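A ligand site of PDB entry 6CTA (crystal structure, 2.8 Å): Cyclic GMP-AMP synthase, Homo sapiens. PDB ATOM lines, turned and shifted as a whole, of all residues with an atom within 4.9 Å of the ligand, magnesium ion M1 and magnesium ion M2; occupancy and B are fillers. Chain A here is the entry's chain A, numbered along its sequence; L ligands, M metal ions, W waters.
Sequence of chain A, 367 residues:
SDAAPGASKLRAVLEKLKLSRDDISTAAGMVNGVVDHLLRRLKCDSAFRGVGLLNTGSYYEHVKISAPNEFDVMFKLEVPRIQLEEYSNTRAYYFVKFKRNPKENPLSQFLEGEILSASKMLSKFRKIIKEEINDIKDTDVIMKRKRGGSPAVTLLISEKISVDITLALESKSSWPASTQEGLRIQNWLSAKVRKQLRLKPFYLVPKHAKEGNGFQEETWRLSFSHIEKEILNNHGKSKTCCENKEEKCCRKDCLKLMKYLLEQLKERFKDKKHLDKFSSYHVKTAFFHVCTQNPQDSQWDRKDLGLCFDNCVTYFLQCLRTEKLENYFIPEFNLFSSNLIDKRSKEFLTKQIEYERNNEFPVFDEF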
ATOM      1  N   THR A  56     -14.553 -23.997   5.539  1.00  0.00           N
ATOM      2  CA  THR A  56     -14.357 -22.976   6.549  1.00  0.00           C
ATOM      3  C   THR A  56     -14.278 -21.603   5.875  1.00  0.00           C
ATOM      4  O   THR A  56     -14.333 -21.486   4.652  1.00  0.00           O
ATOM      5  CB  THR A  56     -13.080 -23.235   7.363  1.00  0.00           C
ATOM      6  OG1 THR A  56     -11.928 -23.010   6.544  1.00  0.00           O
ATOM      7  CG2 THR A  56     -13.057 -24.683   7.861  1.00  0.00           C
ATOM      8  N   GLY A  57     -14.163 -20.571   6.690  1.00  0.00           N
ATOM      9  CA  GLY A  57     -13.890 -19.243   6.174  1.00  0.00           C
ATOM     10  C   GLY A  57     -15.130 -18.434   5.852  1.00  0.00           C
ATOM     11  O   GLY A  57     -16.275 -18.848   6.042  1.00  0.00           O
ATOM     12  N   SER A  58     -14.868 -17.225   5.326  1.00  0.00           N
ATOM     13  CA  SER A  58     -15.915 -16.228   5.150  1.00  0.00           C
ATOM     14  C   SER A  58     -16.970 -16.672   4.133  1.00  0.00           C
ATOM     15  O   SER A  58     -18.160 -16.401   4.309  1.00  0.00           O
ATOM     16  CB  SER A  58     -15.293 -14.902   4.726  1.00  0.00           C
ATOM     17  OG  SER A  58     -14.463 -15.075   3.594  1.00  0.00           O
ATOM     18  N   GLU A  61     -19.286 -19.064   5.614  1.00  0.00           N
ATOM     19  CA  GLU A  61     -19.968 -18.352   6.683  1.00  0.00           C
ATOM     20  C   GLU A  61     -20.880 -17.245   6.157  1.00  0.00           C
ATOM     21  O   GLU A  61     -21.536 -16.571   6.946  1.00  0.00           O
ATOM     22  CB  GLU A  61     -18.951 -17.753   7.658  1.00  0.00           C
ATOM     23  CG  GLU A  61     -18.209 -18.788   8.480  1.00  0.00           C
ATOM     24  CD  GLU A  61     -16.921 -18.238   9.072  1.00  0.00           C
ATOM     25  OE1 GLU A  61     -16.410 -17.223   8.551  1.00  0.00           O
ATOM     26  OE2 GLU A  61     -16.430 -18.820  10.059  1.00  0.00           O
ATOM     27  N   LYS A  64     -18.341 -13.340   3.102  1.00  0.00           N
ATOM     28  CA  LYS A  64     -17.415 -12.919   2.059  1.00  0.00           C
ATOM     29  C   LYS A  64     -17.946 -11.670   1.375  1.00  0.00           C
ATOM     30  O   LYS A  64     -19.155 -11.511   1.191  1.00  0.00           O
ATOM     31  CB  LYS A  64     -17.223 -14.035   1.028  1.00  0.00           C
ATOM     32  CG  LYS A  64     -16.146 -13.765  -0.022  1.00  0.00           C
ATOM     33  CD  LYS A  64     -14.746 -13.984   0.544  1.00  0.00           C
ATOM     34  CE  LYS A  64     -13.678 -13.768  -0.511  1.00  0.00           C
ATOM     35  NZ  LYS A  64     -13.667 -12.374  -1.031  1.00  0.00           N
ATOM     36  N   GLU A  70     -11.775 -15.842  -2.767  1.00  0.00           N
ATOM     37  CA  GLU A  70     -10.938 -16.525  -1.791  1.00  0.00           C
ATOM     38  C   GLU A  70     -11.789 -17.537  -1.034  1.00  0.00           C
ATOM     39  O   GLU A  70     -12.756 -17.163  -0.361  1.00  0.00           O
ATOM     40  CB  GLU A  70     -10.277 -15.539  -0.830  1.00  0.00           C
ATOM     41  CG  GLU A  70      -9.046 -16.083  -0.125  1.00  0.00           C
ATOM     42  CD  GLU A  70      -9.313 -16.486   1.306  1.00  0.00           C
ATOM     43  OE1 GLU A  70     -10.475 -16.391   1.751  1.00  0.00           O
ATOM     44  OE2 GLU A  70      -8.361 -16.892   2.001  1.00  0.00           O
ATOM     45  N   PHE A  71     -11.433 -18.810  -1.157  1.00  0.00           N
ATOM     46  CA  PHE A  71     -12.124 -19.897  -0.472  1.00  0.00           C
ATOM     47  C   PHE A  71     -11.156 -20.549   0.519  1.00  0.00           C
ATOM     48  O   PHE A  71      -9.946 -20.584   0.289  1.00  0.00           O
ATOM     49  CB  PHE A  71     -12.638 -20.955  -1.465  1.00  0.00           C
ATOM     50  CG  PHE A  71     -13.739 -20.456  -2.358  1.00  0.00           C
ATOM     51  CD1 PHE A  71     -13.483 -19.538  -3.361  1.00  0.00           C
ATOM     52  CD2 PHE A  71     -15.036 -20.921  -2.211  1.00  0.00           C
ATOM     53  CE1 PHE A  71     -14.491 -19.083  -4.181  1.00  0.00           C
ATOM     54  CE2 PHE A  71     -16.051 -20.470  -3.029  1.00  0.00           C
ATOM     55  CZ  PHE A  71     -15.777 -19.559  -4.021  1.00  0.00           C
ATOM     56  N   ASP A  72     -11.717 -21.068   1.612  1.00  0.00           N
ATOM     57  CA  ASP A  72     -10.926 -21.719   2.646  1.00  0.00           C
ATOM     58  C   ASP A  72     -11.511 -23.092   2.920  1.00  0.00           C
ATOM     59  O   ASP A  72     -12.655 -23.203   3.368  1.00  0.00           O
ATOM     60  CB  ASP A  72     -10.897 -20.882   3.929  1.00  0.00           C
ATOM     61  CG  ASP A  72     -10.296 -19.509   3.702  1.00  0.00           C
ATOM     62  OD1 ASP A  72      -9.070 -19.413   3.486  1.00  0.00           O
ATOM     63  OD2 ASP A  72     -11.062 -18.525   3.716  1.00  0.00           O
ATOM     64  N   PRO A 151      -2.287 -21.914   6.022  1.00  0.00           N
ATOM     65  CA  PRO A 151      -2.696 -22.963   5.075  1.00  0.00           C
ATOM     66  C   PRO A 151      -1.539 -23.716   4.425  1.00  0.00           C
ATOM     67  O   PRO A 151      -0.510 -23.117   4.111  1.00  0.00           O
ATOM     68  CB  PRO A 151      -3.481 -22.187   4.014  1.00  0.00           C
ATOM     69  CG  PRO A 151      -3.857 -20.894   4.661  1.00  0.00           C
ATOM     70  CD  PRO A 151      -2.717 -20.582   5.573  1.00  0.00           C
ATOM     71  N   ASP A 164      -7.424 -21.604  -0.168  1.00  0.00           N
ATOM     72  CA  ASP A 164      -6.499 -22.013   0.879  1.00  0.00           C
ATOM     73  C   ASP A 164      -6.895 -23.408   1.375  1.00  0.00           C
ATOM     74  O   ASP A 164      -8.026 -23.609   1.818  1.00  0.00           O
ATOM     75  CB  ASP A 164      -6.514 -21.015   2.039  1.00  0.00           C
ATOM     76  CG  ASP A 164      -5.843 -19.702   1.671  1.00  0.00           C
ATOM     77  OD1 ASP A 164      -4.988 -19.697   0.772  1.00  0.00           O
ATOM     78  OD2 ASP A 164      -6.184 -18.665   2.287  1.00  0.00           O
ATOM     79  N   ARG A 221      -1.421 -26.037  15.850  1.00  0.00           N
ATOM     80  CA  ARG A 221      -2.247 -25.014  16.476  1.00  0.00           C
ATOM     81  C   ARG A 221      -3.702 -25.463  16.490  1.00  0.00           C
ATOM     82  O   ARG A 221      -4.179 -26.081  15.541  1.00  0.00           O
ATOM     83  CB  ARG A 221      -2.109 -23.674  15.749  1.00  0.00           C
ATOM     84  CG  ARG A 221      -2.885 -22.535  16.397  1.00  0.00           C
ATOM     85  CD  ARG A 221      -3.852 -21.907  15.402  1.00  0.00           C
ATOM     86  NE  ARG A 221      -3.181 -21.020  14.464  1.00  0.00           N
ATOM     87  CZ  ARG A 221      -3.679 -20.678  13.272  1.00  0.00           C
ATOM     88  NH1 ARG A 221      -4.839 -21.171  12.875  1.00  0.00           N
ATOM     89  NH2 ARG A 221      -3.005 -19.860  12.483  1.00  0.00           N
ATOM     90  N   LEU A 222      -4.394 -25.151  17.583  1.00  0.00           N
ATOM     91  CA  LEU A 222      -5.808 -25.487  17.695  1.00  0.00           C
ATOM     92  C   LEU A 222      -6.628 -24.707  16.679  1.00  0.00           C
ATOM     93  O   LEU A 222      -6.382 -23.528  16.420  1.00  0.00           O
ATOM     94  CB  LEU A 222      -6.325 -25.180  19.106  1.00  0.00           C
ATOM     95  CG  LEU A 222      -5.773 -26.009  20.268  1.00  0.00           C
ATOM     96  CD1 LEU A 222      -6.342 -25.507  21.590  1.00  0.00           C
ATOM     97  CD2 LEU A 222      -6.096 -27.485  20.082  1.00  0.00           C
ATOM     98  N   SER A 225     -12.583 -23.592  13.386  1.00  0.00           N
ATOM     99  CA  SER A 225     -13.261 -22.936  12.273  1.00  0.00           C
ATOM    100  C   SER A 225     -14.657 -23.500  12.054  1.00  0.00           C
ATOM    101  O   SER A 225     -15.558 -22.781  11.603  1.00  0.00           O
ATOM    102  CB  SER A 225     -12.431 -23.086  10.998  1.00  0.00           C
ATOM    103  OG  SER A 225     -11.134 -22.537  11.177  1.00  0.00           O
ATOM    104  N   GLU A 228     -16.782 -21.691  14.491  1.00  0.00           N
ATOM    105  CA  GLU A 228     -16.988 -20.327  14.020  1.00  0.00           C
ATOM    106  C   GLU A 228     -18.039 -20.286  12.917  1.00  0.00           C
ATOM    107  O   GLU A 228     -18.870 -19.371  12.869  1.00  0.00           O
ATOM    108  CB  GLU A 228     -15.672 -19.726  13.540  1.00  0.00           C
ATOM    109  CG  GLU A 228     -14.592 -19.687  14.610  1.00  0.00           C
ATOM    110  CD  GLU A 228     -13.233 -19.322  14.050  1.00  0.00           C
ATOM    111  OE1 GLU A 228     -13.133 -19.073  12.829  1.00  0.00           O
ATOM    112  OE2 GLU A 228     -12.261 -19.281  14.823  1.00  0.00           O
ATOM    113  N   LYS A 259     -14.707  -6.177   8.113  1.00  0.00           N
ATOM    114  CA  LYS A 259     -13.775  -6.790   7.181  1.00  0.00           C
ATOM    115  C   LYS A 259     -13.420  -5.845   6.055  1.00  0.00           C
ATOM    116  O   LYS A 259     -12.262  -5.773   5.623  1.00  0.00           O
ATOM    117  CB  LYS A 259     -14.373  -8.091   6.618  1.00  0.00           C
ATOM    118  CG  LYS A 259     -14.623  -9.175   7.651  1.00  0.00           C
ATOM    119  CD  LYS A 259     -15.426 -10.313   7.056  1.00  0.00           C
ATOM    120  CE  LYS A 259     -14.607 -11.150   6.096  1.00  0.00           C
ATOM    121  NZ  LYS A 259     -13.504 -11.845   6.811  1.00  0.00           N
ATOM    122  N   GLU A 263      -9.826  -4.214   5.093  1.00  0.00           N
ATOM    123  CA  GLU A 263      -9.352  -4.455   3.734  1.00  0.00           C
ATOM    124  C   GLU A 263      -9.034  -3.153   3.021  1.00  0.00           C
ATOM    125  O   GLU A 263      -8.015  -3.048   2.324  1.00  0.00           O
ATOM    126  CB  GLU A 263     -10.384  -5.262   2.948  1.00  0.00           C
ATOM    127  CG  GLU A 263     -10.118  -6.753   2.915  1.00  0.00           C
ATOM    128  CD  GLU A 263     -11.080  -7.499   2.008  1.00  0.00           C
ATOM    129  OE1 GLU A 263     -11.700  -8.477   2.476  1.00  0.00           O
ATOM    130  OE2 GLU A 263     -11.211  -7.101   0.836  1.00  0.00           O
ATOM    131  N   SER A 280      -8.124 -10.462   8.670  1.00  0.00           N
ATOM    132  CA  SER A 280      -9.559 -10.445   8.906  1.00  0.00           C
ATOM    133  C   SER A 280      -9.962 -11.312  10.084  1.00  0.00           C
ATOM    134  O   SER A 280     -11.058 -11.123  10.639  1.00  0.00           O
ATOM    135  CB  SER A 280     -10.310 -10.895   7.647  1.00  0.00           C
ATOM    136  OG  SER A 280      -9.849 -12.155   7.210  1.00  0.00           O
ATOM    137  N   TYR A 281      -9.116 -12.263  10.487  1.00  0.00           N
ATOM    138  CA  TYR A 281      -9.420 -13.076  11.663  1.00  0.00           C
ATOM    139  C   TYR A 281      -9.374 -12.254  12.936  1.00  0.00           C
ATOM    140  O   TYR A 281     -10.109 -12.540  13.883  1.00  0.00           O
ATOM    141  CB  TYR A 281      -8.449 -14.261  11.767  1.00  0.00           C
ATOM    142  CG  TYR A 281      -8.821 -15.241  12.852  1.00  0.00           C
ATOM    143  CD1 TYR A 281      -9.913 -16.097  12.682  1.00  0.00           C
ATOM    144  CD2 TYR A 281      -8.101 -15.325  14.034  1.00  0.00           C
ATOM    145  CE1 TYR A 281     -10.266 -16.996  13.670  1.00  0.00           C
ATOM    146  CE2 TYR A 281      -8.454 -16.223  15.021  1.00  0.00           C
ATOM    147  CZ  TYR A 281      -9.525 -17.061  14.836  1.00  0.00           C
ATOM    148  OH  TYR A 281      -9.882 -17.961  15.810  1.00  0.00           O
ATOM    149  N   LYS A 284     -12.722 -10.781  12.845  1.00  0.00           N
ATOM    150  CA  LYS A 284     -13.746 -11.772  13.134  1.00  0.00           C
ATOM    151  C   LYS A 284     -13.729 -12.173  14.606  1.00  0.00           C
ATOM    152  O   LYS A 284     -14.786 -12.323  15.223  1.00  0.00           O
ATOM    153  CB  LYS A 284     -13.546 -13.011  12.251  1.00  0.00           C
ATOM    154  CG  LYS A 284     -14.710 -13.985  12.321  1.00  0.00           C
ATOM    155  CD  LYS A 284     -14.239 -15.436  12.329  1.00  0.00           C
ATOM    156  CE  LYS A 284     -14.462 -16.106  10.981  1.00  0.00           C
ATOM    157  NZ  LYS A 284     -14.337 -17.592  11.070  1.00  0.00           N
ATOM    158  N   ASN A 327      -8.031 -14.848  21.715  1.00  0.00           N
ATOM    159  CA  ASN A 327      -8.618 -15.888  20.891  1.00  0.00           C
ATOM    160  C   ASN A 327      -9.938 -16.344  21.497  1.00  0.00           C
ATOM    161  O   ASN A 327      -9.986 -16.711  22.679  1.00  0.00           O
ATOM    162  CB  ASN A 327      -7.647 -17.059  20.758  1.00  0.00           C
ATOM    163  CG  ASN A 327      -8.229 -18.217  19.972  1.00  0.00           C
ATOM    164  OD1 ASN A 327      -8.942 -19.059  20.524  1.00  0.00           O
ATOM    165  ND2 ASN A 327      -7.923 -18.282  18.680  1.00  0.00           N
ATOM    166  N   LEU A 335      -3.909 -12.489  20.498  1.00  0.00           N
ATOM    167  CA  LEU A 335      -3.588 -12.250  19.106  1.00  0.00           C
ATOM    168  C   LEU A 335      -2.877 -10.913  18.902  1.00  0.00           C
ATOM    169  O   LEU A 335      -2.144 -10.758  17.915  1.00  0.00           O
ATOM    170  CB  LEU A 335      -4.861 -12.303  18.255  1.00  0.00           C
ATOM    171  CG  LEU A 335      -5.590 -13.645  18.207  1.00  0.00           C
ATOM    172  CD1 LEU A 335      -6.980 -13.493  17.597  1.00  0.00           C
ATOM    173  CD2 LEU A 335      -4.777 -14.668  17.430  1.00  0.00           C
HETATM  174  P1  LIG L   1     -11.668 -13.417   4.388  1.00  0.00           P
HETATM  175  O1  LIG L   1     -10.733 -12.297   4.771  1.00  0.00           O
HETATM  176  O2  LIG L   1     -10.976 -14.586   3.720  1.00  0.00           O
HETATM  177  O3  LIG L   1     -12.941 -12.976   3.707  1.00  0.00           O
HETATM  178  P2  LIG L   1     -11.560 -15.430   6.328  1.00  0.00           P
HETATM  179  O4  LIG L   1     -11.991 -15.608   7.774  1.00  0.00           O
HETATM  180  O5  LIG L   1     -11.901 -16.474   5.306  1.00  0.00           O
HETATM  181  O6  LIG L   1     -12.141 -14.013   5.809  1.00  0.00           O
HETATM  182  P3  LIG L   1      -8.863 -16.335   6.164  1.00  0.00           P
HETATM  183  O7  LIG L   1      -8.995 -16.979   4.813  1.00  0.00           O
HETATM  184  O8  LIG L   1      -7.541 -15.744   6.603  1.00  0.00           O
HETATM  185  O9  LIG L   1      -9.969 -15.165   6.279  1.00  0.00           O
HETATM  186  O10 LIG L   1      -9.278 -17.402   7.301  1.00  0.00           O
HETATM  187  C1  LIG L   1     -10.070 -18.548   6.984  1.00  0.00           C
HETATM  188  C2  LIG L   1     -10.375 -19.296   8.268  1.00  0.00           C
HETATM  189  O11 LIG L   1      -9.167 -19.773   8.867  1.00  0.00           O
HETATM  190  C3  LIG L   1     -11.025 -18.397   9.310  1.00  0.00           C
HETATM  191  O12 LIG L   1     -12.447 -18.459   9.230  1.00  0.00           O
HETATM  192  C4  LIG L   1     -10.524 -18.930  10.632  1.00  0.00           C
HETATM  193  O13 LIG L   1     -11.453 -19.875  11.148  1.00  0.00           O
HETATM  194  C5  LIG L   1      -9.224 -19.650  10.296  1.00  0.00           C
HETATM  195  N1  LIG L   1      -8.092 -18.792  10.742  1.00  0.00           N
HETATM  196  C6  LIG L   1      -7.476 -17.868   9.988  1.00  0.00           C
HETATM  197  N2  LIG L   1      -6.485 -17.254  10.687  1.00  0.00           N
HETATM  198  C7  LIG L   1      -6.474 -17.789  11.916  1.00  0.00           C
HETATM  199  C8  LIG L   1      -5.685 -17.593  13.158  1.00  0.00           C
HETATM  200  N3  LIG L   1      -4.679 -16.672  13.207  1.00  0.00           N
HETATM  201  N4  LIG L   1      -5.990 -18.359  14.225  1.00  0.00           N
HETATM  202  C9  LIG L   1      -6.976 -19.269  14.184  1.00  0.00           C
HETATM  203  N5  LIG L   1      -7.734 -19.495  13.100  1.00  0.00           N
HETATM  204  C10 LIG L   1      -7.533 -18.802  11.952  1.00  0.00           C
HETATM  205 MG    MG M   1     -11.612 -16.711   3.301  1.00  0.00          MG
HETATM  206 MG    MG M   2      -6.726 -17.976   4.487  1.00  0.00          MG
HETATM  207  O   HOH W   1     -11.654  -9.464   4.775  1.00  0.00           O
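An oxygen (O13) of the ligand sits at hydrogen-bond distance from the side-chain carboxylate (OE1) of Glu 228. N of Ser 58 lies close to O5 of the ligand. The side-chain hydroxyl of Ser 58 is in hydrogen-bond range of an oxygen (O3) of the ligand, at 2.6 Å. OG of Ser 280 is in hydrogen-bond range of O1 of the ligand, 2.6 Å away. O13 of the ligand is in hydrogen-bond range of OG of Ser 225 (2.7 Å). NZ of Lys 259 lies within salt-bridge range of O3 of the ligand (3.4 Å). The side-chain amino group (NZ) of Lys 284 lies within hydrogen-bond range of an oxygen (O12) of the ligand (2.8 Å). A nitrogen (N4) of the ligand sits close to the guanidinium group (NH1) of Arg 221 (3.3 Å).
N of Thr 56 is in hydrogen-bond range of O of Asp 72 (3.0 Å). The backbone carbonyl oxygen (O) of Phe 71 lies within hydrogen-bond range of the backbone NH (N) of Asp 164, at 2.8 Å. OE1 of Glu 228 lies within salt-bridge range of NZ of Lys 284 (2.6 Å). The side-chain carboxylate (OE2) of Glu 228 sits at hydrogen-bond distance from the side-chain hydroxyl (OH) of Tyr 281, 2.9 Å away. The backbone carbonyl oxygen of Ser 58 is in hydrogen-bond range of the backbone NH of Lys 64, 3.3 Å away. The side-chain carboxylate (OE2) of Glu 61 is in salt-bridge range of the side-chain amino group (NZ) of Lys 284. OH of Tyr 281 lies within hydrogen-bond range of ND2 of Asn 327.
Merely in contact with the ligand: Tyr 281 (3.4 Å), Gly 57 (3.5 Å) and Lys 64 (3.8 Å). Hydrophobic or aromatic side chains within 4 Å of the ligand: Tyr 281. 12 residues have an atom within 4 Å of the ligand: Gly 57, Ser 58, Lys 64, Glu 70, Asp 72, Arg 221, Ser 225, Glu 228, Lys 259, Ser 280, Tyr 281 and Lys 284.
OG of Ser 58 touches magnesium ion M1 (3.3 Å). The nearest printed residue that does not touch magnesium ion M1 is Gly 57 (4.5 Å).
Within 4 Å of magnesium ion M2: Glu 70, Asp 72 and Asp 164.
Magnesium ion M1 is bound by the side-chain carboxylate of Asp 72, the side-chain carboxylate of Glu 70, an oxygen (O5) of the ligand and an oxygen (O2) of the ligand. Magnesium ion M1 has four donor atoms within binding distance.
Magnesium ion M2 is bound by OD2 of Asp 164 (2.4 Å). Magnesium ion M2 is bound by O7 of the ligand (2.5 Å). Magnesium ion M2 has two donor atoms within binding distance.
Water W1 lies within hydrogen-bond range of the side-chain carboxylate of Glu 263 (2.5 Å) and an oxygen (O1) of the ligand (3.0 Å).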
